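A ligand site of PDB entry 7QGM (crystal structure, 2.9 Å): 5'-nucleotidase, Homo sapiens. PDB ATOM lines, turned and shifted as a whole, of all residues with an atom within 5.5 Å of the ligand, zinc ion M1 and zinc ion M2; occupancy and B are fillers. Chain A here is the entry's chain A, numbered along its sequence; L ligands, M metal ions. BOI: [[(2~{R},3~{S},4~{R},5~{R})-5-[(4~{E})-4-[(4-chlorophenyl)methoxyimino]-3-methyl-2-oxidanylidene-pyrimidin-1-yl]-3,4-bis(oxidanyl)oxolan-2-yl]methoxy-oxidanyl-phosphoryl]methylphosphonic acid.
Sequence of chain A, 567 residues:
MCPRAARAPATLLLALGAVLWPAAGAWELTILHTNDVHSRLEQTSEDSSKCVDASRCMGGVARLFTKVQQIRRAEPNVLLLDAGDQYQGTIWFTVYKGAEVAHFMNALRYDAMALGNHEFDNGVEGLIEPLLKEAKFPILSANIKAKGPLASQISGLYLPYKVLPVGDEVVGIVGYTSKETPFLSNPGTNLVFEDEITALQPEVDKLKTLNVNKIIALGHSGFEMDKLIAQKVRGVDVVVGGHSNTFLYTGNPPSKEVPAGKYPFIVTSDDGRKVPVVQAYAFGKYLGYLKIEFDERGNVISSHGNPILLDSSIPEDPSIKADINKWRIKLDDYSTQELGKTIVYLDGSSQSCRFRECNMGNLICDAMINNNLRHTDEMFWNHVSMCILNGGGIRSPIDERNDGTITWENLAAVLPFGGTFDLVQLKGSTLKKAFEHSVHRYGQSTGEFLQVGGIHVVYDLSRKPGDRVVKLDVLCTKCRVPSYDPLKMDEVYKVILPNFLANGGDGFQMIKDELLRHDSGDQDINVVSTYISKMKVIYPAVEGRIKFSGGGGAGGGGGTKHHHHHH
OD2 of Asp 506 sits at hydrogen-bond distance from O9 of the ligand.
The guanidinium group of Arg 395 lies within salt-bridge range of an oxygen (O) of the ligand.
An oxygen (O9) of the ligand is in hydrogen-bond range of the side-chain amide nitrogen (ND2) of Asn 390.
A ring nitrogen (NE2) of His 118 sits at hydrogen-bond distance from an oxygen (O1) of the ligand, 3.0 Å away.
O of Gly 447 lies within hydrogen-bond range of O9 of the ligand (3.1 Å).
NH1 of Arg 354 lies within salt-bridge range of O3 of the ligand, at 3.4 Å.
The backbone carbonyl oxygen (O) of Asn 117 is in hydrogen-bond range of the side-chain hydroxyl (OG) of Ser 185 (2.8 Å).
The side-chain amide nitrogen of Asn 390 sits close to the backbone NH of Gly 393 (3.0 Å).
ND1 of His 118 sits at hydrogen-bond distance from OD2 of Asp 121, at 2.9 Å.
OD1 of Asn 245 lies close to OD2 of Asp 36 (3.2 Å).
NH2 of Arg 354 lies within hydrogen-bond range of O of Gly 392 (3.3 Å).
The backbone carbonyl oxygen (O) of Ser 445 lies within hydrogen-bond range of the guanidinium group (NH1) of Arg 354 (3.4 Å).
OD2 of Asp 121 sits close to NE2 of Gln 88 (3.3 Å).
The backbone carbonyl oxygen (O) of Asp 121 sits at hydrogen-bond distance from the side-chain amide nitrogen (ND2) of Asn 186.
O of Leu 184 sits close to O7 of the ligand (3.3 Å).
Gln 88 touches the ligand (NE2 to CL, 3.5 Å).
OD1 of Asp 121 touches C12 of the ligand, 3.5 Å away.
Asn 186 touches the ligand.
Asn 245 touches the ligand.
Gly 392 touches the ligand (CA to O9, 3.3 Å).
CA of Gly 393 touches O8 of the ligand, 3.4 Å away.
Phe 417 touches the ligand.
Phe 500 touches the ligand.
Of the 28 residues printed, 19 come within 4 Å of the ligand.
Asp 36 touches zinc ion M1.
OD1 of Asn 245 touches zinc ion M1, 3.3 Å away.
Within 4 Å of zinc ion M1: Asp 36, His 38, Asp 85 and Asn 245.
The nearest printed residue that does not touch zinc ion M1 is His 243 (4.7 Å).
CD2 of His 118 touches zinc ion M2, at 3.8 Å.
Of the 28 residues printed, 5 come within 4 Å of zinc ion M2.
The nearest printed residue that does not touch zinc ion M2 is Asp 36 (4.7 Å).
Zinc ion M1 is bound by OD2 of Asp 85 (2.3 Å) and NE2 of His 38 (2.3 Å).
Zinc ion M1 has two donor atoms within binding distance.
Zinc ion M2 is bound by O2 of the ligand, at 1.8 Å.
Zinc ion M2 is bound by OD1 of Asn 117.
Zinc ion M2 is bound by a ring nitrogen (NE2) of His 220 (2.3 Å).
A ring nitrogen (ND1) of His 243 binds zinc ion M2 (2.3 Å).
The side-chain carboxylate (OD2) of Asp 85 binds zinc ion M2, at 2.4 Å.
Slightly farther from zinc ion M2 lies OD1 of Asp 85 (2.8 Å).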
ATOM      1  N   ASP A  36      26.100 -14.750  -7.276  1.00  0.00           N
ATOM      2  CA  ASP A  36      25.797 -15.687  -6.199  1.00  0.00           C
ATOM      3  C   ASP A  36      25.506 -14.942  -4.889  1.00  0.00           C
ATOM      4  O   ASP A  36      26.063 -15.262  -3.837  1.00  0.00           O
ATOM      5  CB  ASP A  36      26.934 -16.692  -6.016  1.00  0.00           C
ATOM      6  CG  ASP A  36      27.415 -17.262  -7.341  1.00  0.00           C
ATOM      7  OD1 ASP A  36      26.567 -17.718  -8.145  1.00  0.00           O
ATOM      8  OD2 ASP A  36      28.645 -17.254  -7.586  1.00  0.00           O
ATOM      9  N   HIS A  38      22.433 -14.823  -3.497  1.00  0.00           N
ATOM     10  CA  HIS A  38      21.532 -15.727  -2.777  1.00  0.00           C
ATOM     11  C   HIS A  38      20.727 -14.973  -1.712  1.00  0.00           C
ATOM     12  O   HIS A  38      20.665 -15.380  -0.551  1.00  0.00           O
ATOM     13  CB  HIS A  38      22.298 -16.895  -2.179  1.00  0.00           C
ATOM     14  CG  HIS A  38      22.815 -17.861  -3.204  1.00  0.00           C
ATOM     15  ND1 HIS A  38      21.982 -18.516  -4.098  1.00  0.00           N
ATOM     16  CD2 HIS A  38      24.072 -18.291  -3.482  1.00  0.00           C
ATOM     17  CE1 HIS A  38      22.711 -19.294  -4.878  1.00  0.00           C
ATOM     18  NE2 HIS A  38      23.976 -19.174  -4.525  1.00  0.00           N
ATOM     19  N   ASP A  85      22.312 -16.327  -9.828  1.00  0.00           N
ATOM     20  CA  ASP A  85      22.122 -16.777  -8.450  1.00  0.00           C
ATOM     21  C   ASP A  85      21.865 -15.611  -7.496  1.00  0.00           C
ATOM     22  O   ASP A  85      22.674 -15.261  -6.645  1.00  0.00           O
ATOM     23  CB  ASP A  85      23.325 -17.603  -7.974  1.00  0.00           C
ATOM     24  CG  ASP A  85      23.122 -19.101  -8.120  1.00  0.00           C
ATOM     25  OD1 ASP A  85      22.196 -19.525  -8.855  1.00  0.00           O
ATOM     26  OD2 ASP A  85      23.896 -19.869  -7.510  1.00  0.00           O
ATOM     27  N   GLN A  88      17.049 -17.782  -3.596  1.00  0.00           N
ATOM     28  CA  GLN A  88      17.328 -18.707  -2.506  1.00  0.00           C
ATOM     29  C   GLN A  88      18.354 -18.143  -1.528  1.00  0.00           C
ATOM     30  O   GLN A  88      18.670 -16.937  -1.574  1.00  0.00           O
ATOM     31  CB  GLN A  88      17.813 -20.053  -3.047  1.00  0.00           C
ATOM     32  CG  GLN A  88      16.684 -21.070  -3.248  1.00  0.00           C
ATOM     33  CD  GLN A  88      17.173 -22.495  -3.118  1.00  0.00           C
ATOM     34  OE1 GLN A  88      18.351 -22.746  -2.885  1.00  0.00           O
ATOM     35  NE2 GLN A  88      16.255 -23.457  -3.256  1.00  0.00           N
ATOM     36  N   ASN A 117      20.879 -20.696 -12.285  1.00  0.00           N
ATOM     37  CA  ASN A 117      20.114 -21.918 -12.113  1.00  0.00           C
ATOM     38  C   ASN A 117      19.097 -21.786 -10.994  1.00  0.00           C
ATOM     39  O   ASN A 117      18.021 -22.394 -11.054  1.00  0.00           O
ATOM     40  CB  ASN A 117      21.046 -23.098 -11.859  1.00  0.00           C
ATOM     41  CG  ASN A 117      21.491 -23.198 -10.415  1.00  0.00           C
ATOM     42  OD1 ASN A 117      22.391 -22.489  -9.979  1.00  0.00           O
ATOM     43  ND2 ASN A 117      20.849 -24.099  -9.666  1.00  0.00           N
ATOM     44  N   HIS A 118      19.399 -20.993  -9.966  1.00  0.00           N
ATOM     45  CA  HIS A 118      18.492 -20.821  -8.837  1.00  0.00           C
ATOM     46  C   HIS A 118      17.294 -19.947  -9.147  1.00  0.00           C
ATOM     47  O   HIS A 118      16.343 -19.918  -8.358  1.00  0.00           O
ATOM     48  CB  HIS A 118      19.244 -20.250  -7.633  1.00  0.00           C
ATOM     49  CG  HIS A 118      19.955 -21.284  -6.815  1.00  0.00           C
ATOM     50  ND1 HIS A 118      19.649 -21.529  -5.496  1.00  0.00           N
ATOM     51  CD2 HIS A 118      20.942 -22.148  -7.138  1.00  0.00           C
ATOM     52  CE1 HIS A 118      20.423 -22.490  -5.029  1.00  0.00           C
ATOM     53  NE2 HIS A 118      21.217 -22.888  -6.015  1.00  0.00           N
ATOM     54  N   ASP A 121      14.161 -22.164  -9.132  1.00  0.00           N
ATOM     55  CA  ASP A 121      13.806 -22.987  -7.970  1.00  0.00           C
ATOM     56  C   ASP A 121      12.339 -22.837  -7.614  1.00  0.00           C
ATOM     57  O   ASP A 121      11.743 -23.760  -7.042  1.00  0.00           O
ATOM     58  CB  ASP A 121      14.687 -22.619  -6.777  1.00  0.00           C
ATOM     59  CG  ASP A 121      16.154 -22.934  -7.001  1.00  0.00           C
ATOM     60  OD1 ASP A 121      16.471 -23.764  -7.876  1.00  0.00           O
ATOM     61  OD2 ASP A 121      17.001 -22.343  -6.302  1.00  0.00           O
ATOM     62  N   ASN A 122      11.730 -21.695  -7.934  1.00  0.00           N
ATOM     63  CA  ASN A 122      10.303 -21.488  -7.731  1.00  0.00           C
ATOM     64  C   ASN A 122       9.504 -21.731  -9.002  1.00  0.00           C
ATOM     65  O   ASN A 122       8.289 -21.498  -9.012  1.00  0.00           O
ATOM     66  CB  ASN A 122      10.040 -20.093  -7.189  1.00  0.00           C
ATOM     67  CG  ASN A 122       9.822 -20.073  -5.687  1.00  0.00           C
ATOM     68  OD1 ASN A 122       8.787 -19.620  -5.204  1.00  0.00           O
ATOM     69  ND2 ASN A 122      10.793 -20.596  -4.948  1.00  0.00           N
ATOM     70  N   LEU A 184      19.450 -29.483 -11.931  1.00  0.00           N
ATOM     71  CA  LEU A 184      19.803 -28.797 -10.677  1.00  0.00           C
ATOM     72  C   LEU A 184      18.670 -27.961 -10.109  1.00  0.00           C
ATOM     73  O   LEU A 184      18.716 -27.619  -8.925  1.00  0.00           O
ATOM     74  CB  LEU A 184      21.020 -27.893 -10.903  1.00  0.00           C
ATOM     75  CG  LEU A 184      22.230 -28.112 -10.012  1.00  0.00           C
ATOM     76  CD1 LEU A 184      23.510 -27.748 -10.763  1.00  0.00           C
ATOM     77  CD2 LEU A 184      22.106 -27.297  -8.729  1.00  0.00           C
ATOM     78  N   SER A 185      17.661 -27.599 -10.904  1.00  0.00           N
ATOM     79  CA  SER A 185      16.614 -26.679 -10.485  1.00  0.00           C
ATOM     80  C   SER A 185      15.294 -27.216 -11.045  1.00  0.00           C
ATOM     81  O   SER A 185      15.200 -28.389 -11.436  1.00  0.00           O
ATOM     82  CB  SER A 185      16.929 -25.253 -10.953  1.00  0.00           C
ATOM     83  OG  SER A 185      16.021 -24.317 -10.403  1.00  0.00           O
ATOM     84  N   ASN A 186      14.272 -26.368 -11.091  1.00  0.00           N
ATOM     85  CA  ASN A 186      12.940 -26.739 -11.580  1.00  0.00           C
ATOM     86  C   ASN A 186      12.502 -25.766 -12.665  1.00  0.00           C
ATOM     87  O   ASN A 186      11.621 -24.923 -12.441  1.00  0.00           O
ATOM     88  CB  ASN A 186      11.923 -26.766 -10.438  1.00  0.00           C
ATOM     89  CG  ASN A 186      12.494 -27.278  -9.134  1.00  0.00           C
ATOM     90  OD1 ASN A 186      13.049 -28.380  -9.068  1.00  0.00           O
ATOM     91  ND2 ASN A 186      12.369 -26.482  -8.074  1.00  0.00           N
ATOM     92  N   HIS A 220      26.301 -18.010 -16.037  1.00  0.00           N
ATOM     93  CA  HIS A 220      26.221 -18.758 -14.783  1.00  0.00           C
ATOM     94  C   HIS A 220      26.492 -20.228 -15.098  1.00  0.00           C
ATOM     95  O   HIS A 220      25.563 -21.033 -15.189  1.00  0.00           O
ATOM     96  CB  HIS A 220      24.852 -18.550 -14.154  1.00  0.00           C
ATOM     97  CG  HIS A 220      24.735 -19.036 -12.749  1.00  0.00           C
ATOM     98  ND1 HIS A 220      25.232 -18.321 -11.681  1.00  0.00           N
ATOM     99  CD2 HIS A 220      24.167 -20.154 -12.232  1.00  0.00           C
ATOM    100  CE1 HIS A 220      24.983 -18.989 -10.564  1.00  0.00           C
ATOM    101  NE2 HIS A 220      24.342 -20.103 -10.875  1.00  0.00           N
ATOM    102  N   HIS A 243      28.547 -19.045 -10.541  1.00  0.00           N
ATOM    103  CA  HIS A 243      27.942 -20.335 -10.236  1.00  0.00           C
ATOM    104  C   HIS A 243      28.866 -21.304  -9.503  1.00  0.00           C
ATOM    105  O   HIS A 243      28.371 -22.282  -8.935  1.00  0.00           O
ATOM    106  CB  HIS A 243      27.429 -21.079 -11.494  1.00  0.00           C
ATOM    107  CG  HIS A 243      26.835 -22.419 -11.197  1.00  0.00           C
ATOM    108  ND1 HIS A 243      25.659 -22.561 -10.508  1.00  0.00           N
ATOM    109  CD2 HIS A 243      27.265 -23.670 -11.471  1.00  0.00           C
ATOM    110  CE1 HIS A 243      25.371 -23.844 -10.381  1.00  0.00           C
ATOM    111  NE2 HIS A 243      26.334 -24.544 -10.954  1.00  0.00           N
ATOM    112  N   ASN A 245      31.181 -19.825  -7.243  1.00  0.00           N
ATOM    113  CA  ASN A 245      31.590 -18.981  -6.123  1.00  0.00           C
ATOM    114  C   ASN A 245      33.111 -18.952  -6.014  1.00  0.00           C
ATOM    115  O   ASN A 245      33.706 -19.335  -5.008  1.00  0.00           O
ATOM    116  CB  ASN A 245      30.935 -19.454  -4.829  1.00  0.00           C
ATOM    117  CG  ASN A 245      29.469 -19.841  -5.017  1.00  0.00           C
ATOM    118  OD1 ASN A 245      28.572 -18.995  -4.950  1.00  0.00           O
ATOM    119  ND2 ASN A 245      29.224 -21.119  -5.256  1.00  0.00           N
ATOM    120  N   ARG A 354      32.165 -29.884   2.655  1.00  0.00           N
ATOM    121  CA  ARG A 354      32.454 -30.604   1.415  1.00  0.00           C
ATOM    122  C   ARG A 354      33.893 -31.116   1.388  1.00  0.00           C
ATOM    123  O   ARG A 354      34.345 -31.586   0.338  1.00  0.00           O
ATOM    124  CB  ARG A 354      32.183 -29.707   0.209  1.00  0.00           C
ATOM    125  CG  ARG A 354      30.724 -29.282   0.072  1.00  0.00           C
ATOM    126  CD  ARG A 354      30.595 -27.921  -0.608  1.00  0.00           C
ATOM    127  NE  ARG A 354      29.245 -27.381  -0.515  1.00  0.00           N
ATOM    128  CZ  ARG A 354      28.527 -26.966  -1.557  1.00  0.00           C
ATOM    129  NH1 ARG A 354      29.017 -26.974  -2.789  1.00  0.00           N
ATOM    130  NH2 ARG A 354      27.298 -26.502  -1.342  1.00  0.00           N
ATOM    131  N   ASN A 390      24.378 -35.208   1.738  1.00  0.00           N
ATOM    132  CA  ASN A 390      25.285 -34.491   0.852  1.00  0.00           C
ATOM    133  C   ASN A 390      25.588 -33.123   1.437  1.00  0.00           C
ATOM    134  O   ASN A 390      24.674 -32.313   1.638  1.00  0.00           O
ATOM    135  CB  ASN A 390      24.691 -34.369  -0.555  1.00  0.00           C
ATOM    136  CG  ASN A 390      23.388 -33.562  -0.583  1.00  0.00           C
ATOM    137  OD1 ASN A 390      22.347 -34.028  -0.116  1.00  0.00           O
ATOM    138  ND2 ASN A 390      23.447 -32.372  -1.162  1.00  0.00           N
ATOM    139  N   GLY A 391      26.866 -32.842   1.698  1.00  0.00           N
ATOM    140  CA  GLY A 391      27.241 -31.563   2.269  1.00  0.00           C
ATOM    141  C   GLY A 391      26.790 -30.381   1.443  1.00  0.00           C
ATOM    142  O   GLY A 391      26.645 -29.277   1.983  1.00  0.00           O
ATOM    143  N   GLY A 392      26.559 -30.591   0.146  1.00  0.00           N
ATOM    144  CA  GLY A 392      26.053 -29.517  -0.682  1.00  0.00           C
ATOM    145  C   GLY A 392      24.705 -29.001  -0.237  1.00  0.00           C
ATOM    146  O   GLY A 392      24.398 -27.810  -0.417  1.00  0.00           O
ATOM    147  N   GLY A 393      23.870 -29.859   0.350  1.00  0.00           N
ATOM    148  CA  GLY A 393      22.592 -29.408   0.850  1.00  0.00           C
ATOM    149  C   GLY A 393      22.718 -28.406   1.976  1.00  0.00           C
ATOM    150  O   GLY A 393      21.824 -27.574   2.173  1.00  0.00           O
ATOM    151  N   ARG A 395      23.787 -25.171   3.363  1.00  0.00           N
ATOM    152  CA  ARG A 395      24.052 -23.944   2.640  1.00  0.00           C
ATOM    153  C   ARG A 395      24.400 -22.755   3.521  1.00  0.00           C
ATOM    154  O   ARG A 395      24.698 -21.675   2.981  1.00  0.00           O
ATOM    155  CB  ARG A 395      22.845 -23.582   1.754  1.00  0.00           C
ATOM    156  CG  ARG A 395      22.651 -24.497   0.552  1.00  0.00           C
ATOM    157  CD  ARG A 395      23.915 -24.570  -0.293  1.00  0.00           C
ATOM    158  NE  ARG A 395      23.715 -25.301  -1.536  1.00  0.00           N
ATOM    159  CZ  ARG A 395      23.368 -24.746  -2.685  1.00  0.00           C
ATOM    160  NH1 ARG A 395      23.118 -23.446  -2.790  1.00  0.00           N
ATOM    161  NH2 ARG A 395      23.249 -25.514  -3.770  1.00  0.00           N
ATOM    162  N   PRO A 416      17.651 -24.198   2.272  1.00  0.00           N
ATOM    163  CA  PRO A 416      16.711 -23.438   1.435  1.00  0.00           C
ATOM    164  C   PRO A 416      15.830 -24.295   0.544  1.00  0.00           C
ATOM    165  O   PRO A 416      14.822 -23.790   0.028  1.00  0.00           O
ATOM    166  CB  PRO A 416      17.630 -22.536   0.600  1.00  0.00           C
ATOM    167  CG  PRO A 416      18.912 -23.322   0.503  1.00  0.00           C
ATOM    168  CD  PRO A 416      19.055 -24.028   1.837  1.00  0.00           C
ATOM    169  N   PHE A 417      16.175 -25.570   0.352  1.00  0.00           N
ATOM    170  CA  PHE A 417      15.482 -26.374  -0.654  1.00  0.00           C
ATOM    171  C   PHE A 417      14.106 -26.813  -0.178  1.00  0.00           C
ATOM    172  O   PHE A 417      13.162 -26.896  -0.980  1.00  0.00           O
ATOM    173  CB  PHE A 417      16.338 -27.590  -1.008  1.00  0.00           C
ATOM    174  CG  PHE A 417      17.761 -27.242  -1.329  1.00  0.00           C
ATOM    175  CD1 PHE A 417      18.130 -26.892  -2.619  1.00  0.00           C
ATOM    176  CD2 PHE A 417      18.732 -27.265  -0.345  1.00  0.00           C
ATOM    177  CE1 PHE A 417      19.447 -26.577  -2.913  1.00  0.00           C
ATOM    178  CE2 PHE A 417      20.048 -26.951  -0.638  1.00  0.00           C
ATOM    179  CZ  PHE A 417      20.403 -26.610  -1.925  1.00  0.00           C
ATOM    180  N   SER A 445      35.564 -28.392  -4.172  1.00  0.00           N
ATOM    181  CA  SER A 445      34.415 -27.866  -3.436  1.00  0.00           C
ATOM    182  C   SER A 445      33.142 -28.616  -3.823  1.00  0.00           C
ATOM    183  O   SER A 445      32.039 -28.054  -3.797  1.00  0.00           O
ATOM    184  CB  SER A 445      34.257 -26.361  -3.652  1.00  0.00           C
ATOM    185  OG  SER A 445      33.344 -25.795  -2.721  1.00  0.00           O
ATOM    186  N   THR A 446      33.301 -29.889  -4.176  1.00  0.00           N
ATOM    187  CA  THR A 446      32.219 -30.666  -4.744  1.00  0.00           C
ATOM    188  C   THR A 446      31.127 -30.902  -3.710  1.00  0.00           C
ATOM    189  O   THR A 446      31.411 -31.318  -2.582  1.00  0.00           O
ATOM    190  CB  THR A 446      32.754 -31.987  -5.268  1.00  0.00           C
ATOM    191  OG1 THR A 446      33.452 -32.660  -4.207  1.00  0.00           O
ATOM    192  CG2 THR A 446      33.717 -31.748  -6.427  1.00  0.00           C
ATOM    193  N   GLY A 447      29.884 -30.659  -4.103  1.00  0.00           N
ATOM    194  CA  GLY A 447      28.766 -30.727  -3.186  1.00  0.00           C
ATOM    195  C   GLY A 447      28.254 -32.123  -2.881  1.00  0.00           C
ATOM    196  O   GLY A 447      27.432 -32.263  -1.967  1.00  0.00           O
ATOM    197  N   GLU A 448      28.724 -33.147  -3.595  1.00  0.00           N
ATOM    198  CA  GLU A 448      28.267 -34.506  -3.376  1.00  0.00           C
ATOM    199  C   GLU A 448      29.032 -35.221  -2.264  1.00  0.00           C
ATOM    200  O   GLU A 448      28.803 -36.411  -2.035  1.00  0.00           O
ATOM    201  CB  GLU A 448      28.339 -35.317  -4.688  1.00  0.00           C
ATOM    202  CG  GLU A 448      29.716 -35.843  -5.098  1.00  0.00           C
ATOM    203  CD  GLU A 448      30.586 -34.795  -5.743  1.00  0.00           C
ATOM    204  OE1 GLU A 448      30.057 -33.733  -6.138  1.00  0.00           O
ATOM    205  OE2 GLU A 448      31.811 -35.034  -5.869  1.00  0.00           O
ATOM    206  N   PHE A 500      16.286 -35.549  -2.142  1.00  0.00           N
ATOM    207  CA  PHE A 500      17.156 -35.273  -3.287  1.00  0.00           C
ATOM    208  C   PHE A 500      18.173 -36.405  -3.494  1.00  0.00           C
ATOM    209  O   PHE A 500      18.502 -36.743  -4.637  1.00  0.00           O
ATOM    210  CB  PHE A 500      17.837 -33.918  -3.083  1.00  0.00           C
ATOM    211  CG  PHE A 500      19.072 -33.712  -3.916  1.00  0.00           C
ATOM    212  CD1 PHE A 500      18.983 -33.516  -5.283  1.00  0.00           C
ATOM    213  CD2 PHE A 500      20.321 -33.694  -3.310  1.00  0.00           C
ATOM    214  CE1 PHE A 500      20.132 -33.334  -6.035  1.00  0.00           C
ATOM    215  CE2 PHE A 500      21.461 -33.509  -4.060  1.00  0.00           C
ATOM    216  CZ  PHE A 500      21.366 -33.326  -5.426  1.00  0.00           C
ATOM    217  N   ASP A 506      22.921 -35.649  -7.541  1.00  0.00           N
ATOM    218  CA  ASP A 506      24.349 -35.355  -7.425  1.00  0.00           C
ATOM    219  C   ASP A 506      25.230 -36.390  -8.109  1.00  0.00           C
ATOM    220  O   ASP A 506      26.455 -36.335  -7.973  1.00  0.00           O
ATOM    221  CB  ASP A 506      24.761 -35.229  -5.951  1.00  0.00           C
ATOM    222  CG  ASP A 506      25.253 -33.849  -5.596  1.00  0.00           C
ATOM    223  OD1 ASP A 506      25.743 -33.142  -6.504  1.00  0.00           O
ATOM    224  OD2 ASP A 506      25.145 -33.468  -4.416  1.00  0.00           O
HETATM  225  O8  BOI L   1      21.185 -30.267  -2.135  1.00  0.00           O
HETATM  226  C15 BOI L   1      20.856 -29.939  -3.259  1.00  0.00           C
HETATM  227  N2  BOI L   1      19.530 -29.992  -3.677  1.00  0.00           N
HETATM  228  C14 BOI L   1      18.537 -30.397  -2.679  1.00  0.00           C
HETATM  229  C6  BOI L   1      19.098 -29.703  -4.966  1.00  0.00           C
HETATM  230  N1  BOI L   1      17.830 -29.834  -5.172  1.00  0.00           N
HETATM  231  O7  BOI L   1      17.482 -29.519  -6.513  1.00  0.00           O
HETATM  232  C7  BOI L   1      16.062 -29.672  -6.640  1.00  0.00           C
HETATM  233  C8  BOI L   1      15.348 -28.514  -6.014  1.00  0.00           C
HETATM  234  C13 BOI L   1      15.699 -27.199  -6.333  1.00  0.00           C
HETATM  235  C12 BOI L   1      15.058 -26.132  -5.750  1.00  0.00           C
HETATM  236  C11 BOI L   1      14.052 -26.359  -4.844  1.00  0.00           C
HETATM  237 CL   BOI L   1      13.253 -25.013  -4.088  1.00  0.00          CL
HETATM  238  C10 BOI L   1      13.675 -27.641  -4.507  1.00  0.00           C
HETATM  239  C9  BOI L   1      14.326 -28.712  -5.092  1.00  0.00           C
HETATM  240  C5  BOI L   1      20.100 -29.300  -5.893  1.00  0.00           C
HETATM  241  C4  BOI L   1      21.378 -29.237  -5.498  1.00  0.00           C
HETATM  242  N   BOI L   1      21.770 -29.533  -4.219  1.00  0.00           N
HETATM  243  C3  BOI L   1      23.184 -29.447  -3.816  1.00  0.00           C
HETATM  244  O6  BOI L   1      23.721 -28.233  -4.307  1.00  0.00           O
HETATM  245  C16 BOI L   1      24.048 -30.595  -4.373  1.00  0.00           C
HETATM  246  O9  BOI L   1      24.811 -31.165  -3.313  1.00  0.00           O
HETATM  247  C17 BOI L   1      24.950 -29.895  -5.392  1.00  0.00           C
HETATM  248  O10 BOI L   1      26.244 -30.488  -5.488  1.00  0.00           O
HETATM  249  C2  BOI L   1      25.038 -28.479  -4.837  1.00  0.00           C
HETATM  250  C1  BOI L   1      25.408 -27.415  -5.833  1.00  0.00           C
HETATM  251  O5  BOI L   1      25.777 -26.207  -5.119  1.00  0.00           O
HETATM  252  P1  BOI L   1      26.923 -25.258  -5.623  1.00  0.00           P
HETATM  253  O3  BOI L   1      28.193 -25.984  -5.976  1.00  0.00           O
HETATM  254  O4  BOI L   1      27.240 -24.308  -4.431  1.00  0.00           O
HETATM  255  C   BOI L   1      26.131 -24.239  -6.884  1.00  0.00           C
HETATM  256  P   BOI L   1      24.531 -23.524  -6.460  1.00  0.00           P
HETATM  257  O   BOI L   1      24.514 -22.842  -5.131  1.00  0.00           O
HETATM  258  O2  BOI L   1      24.157 -22.563  -7.609  1.00  0.00           O
HETATM  259  O1  BOI L   1      23.531 -24.696  -6.520  1.00  0.00           O
HETATM  260 ZN    ZN M   1      25.595 -19.994  -5.952  1.00  0.00          ZN
HETATM  261 ZN    ZN M   2      24.119 -21.568  -9.123  1.00  0.00          ZN
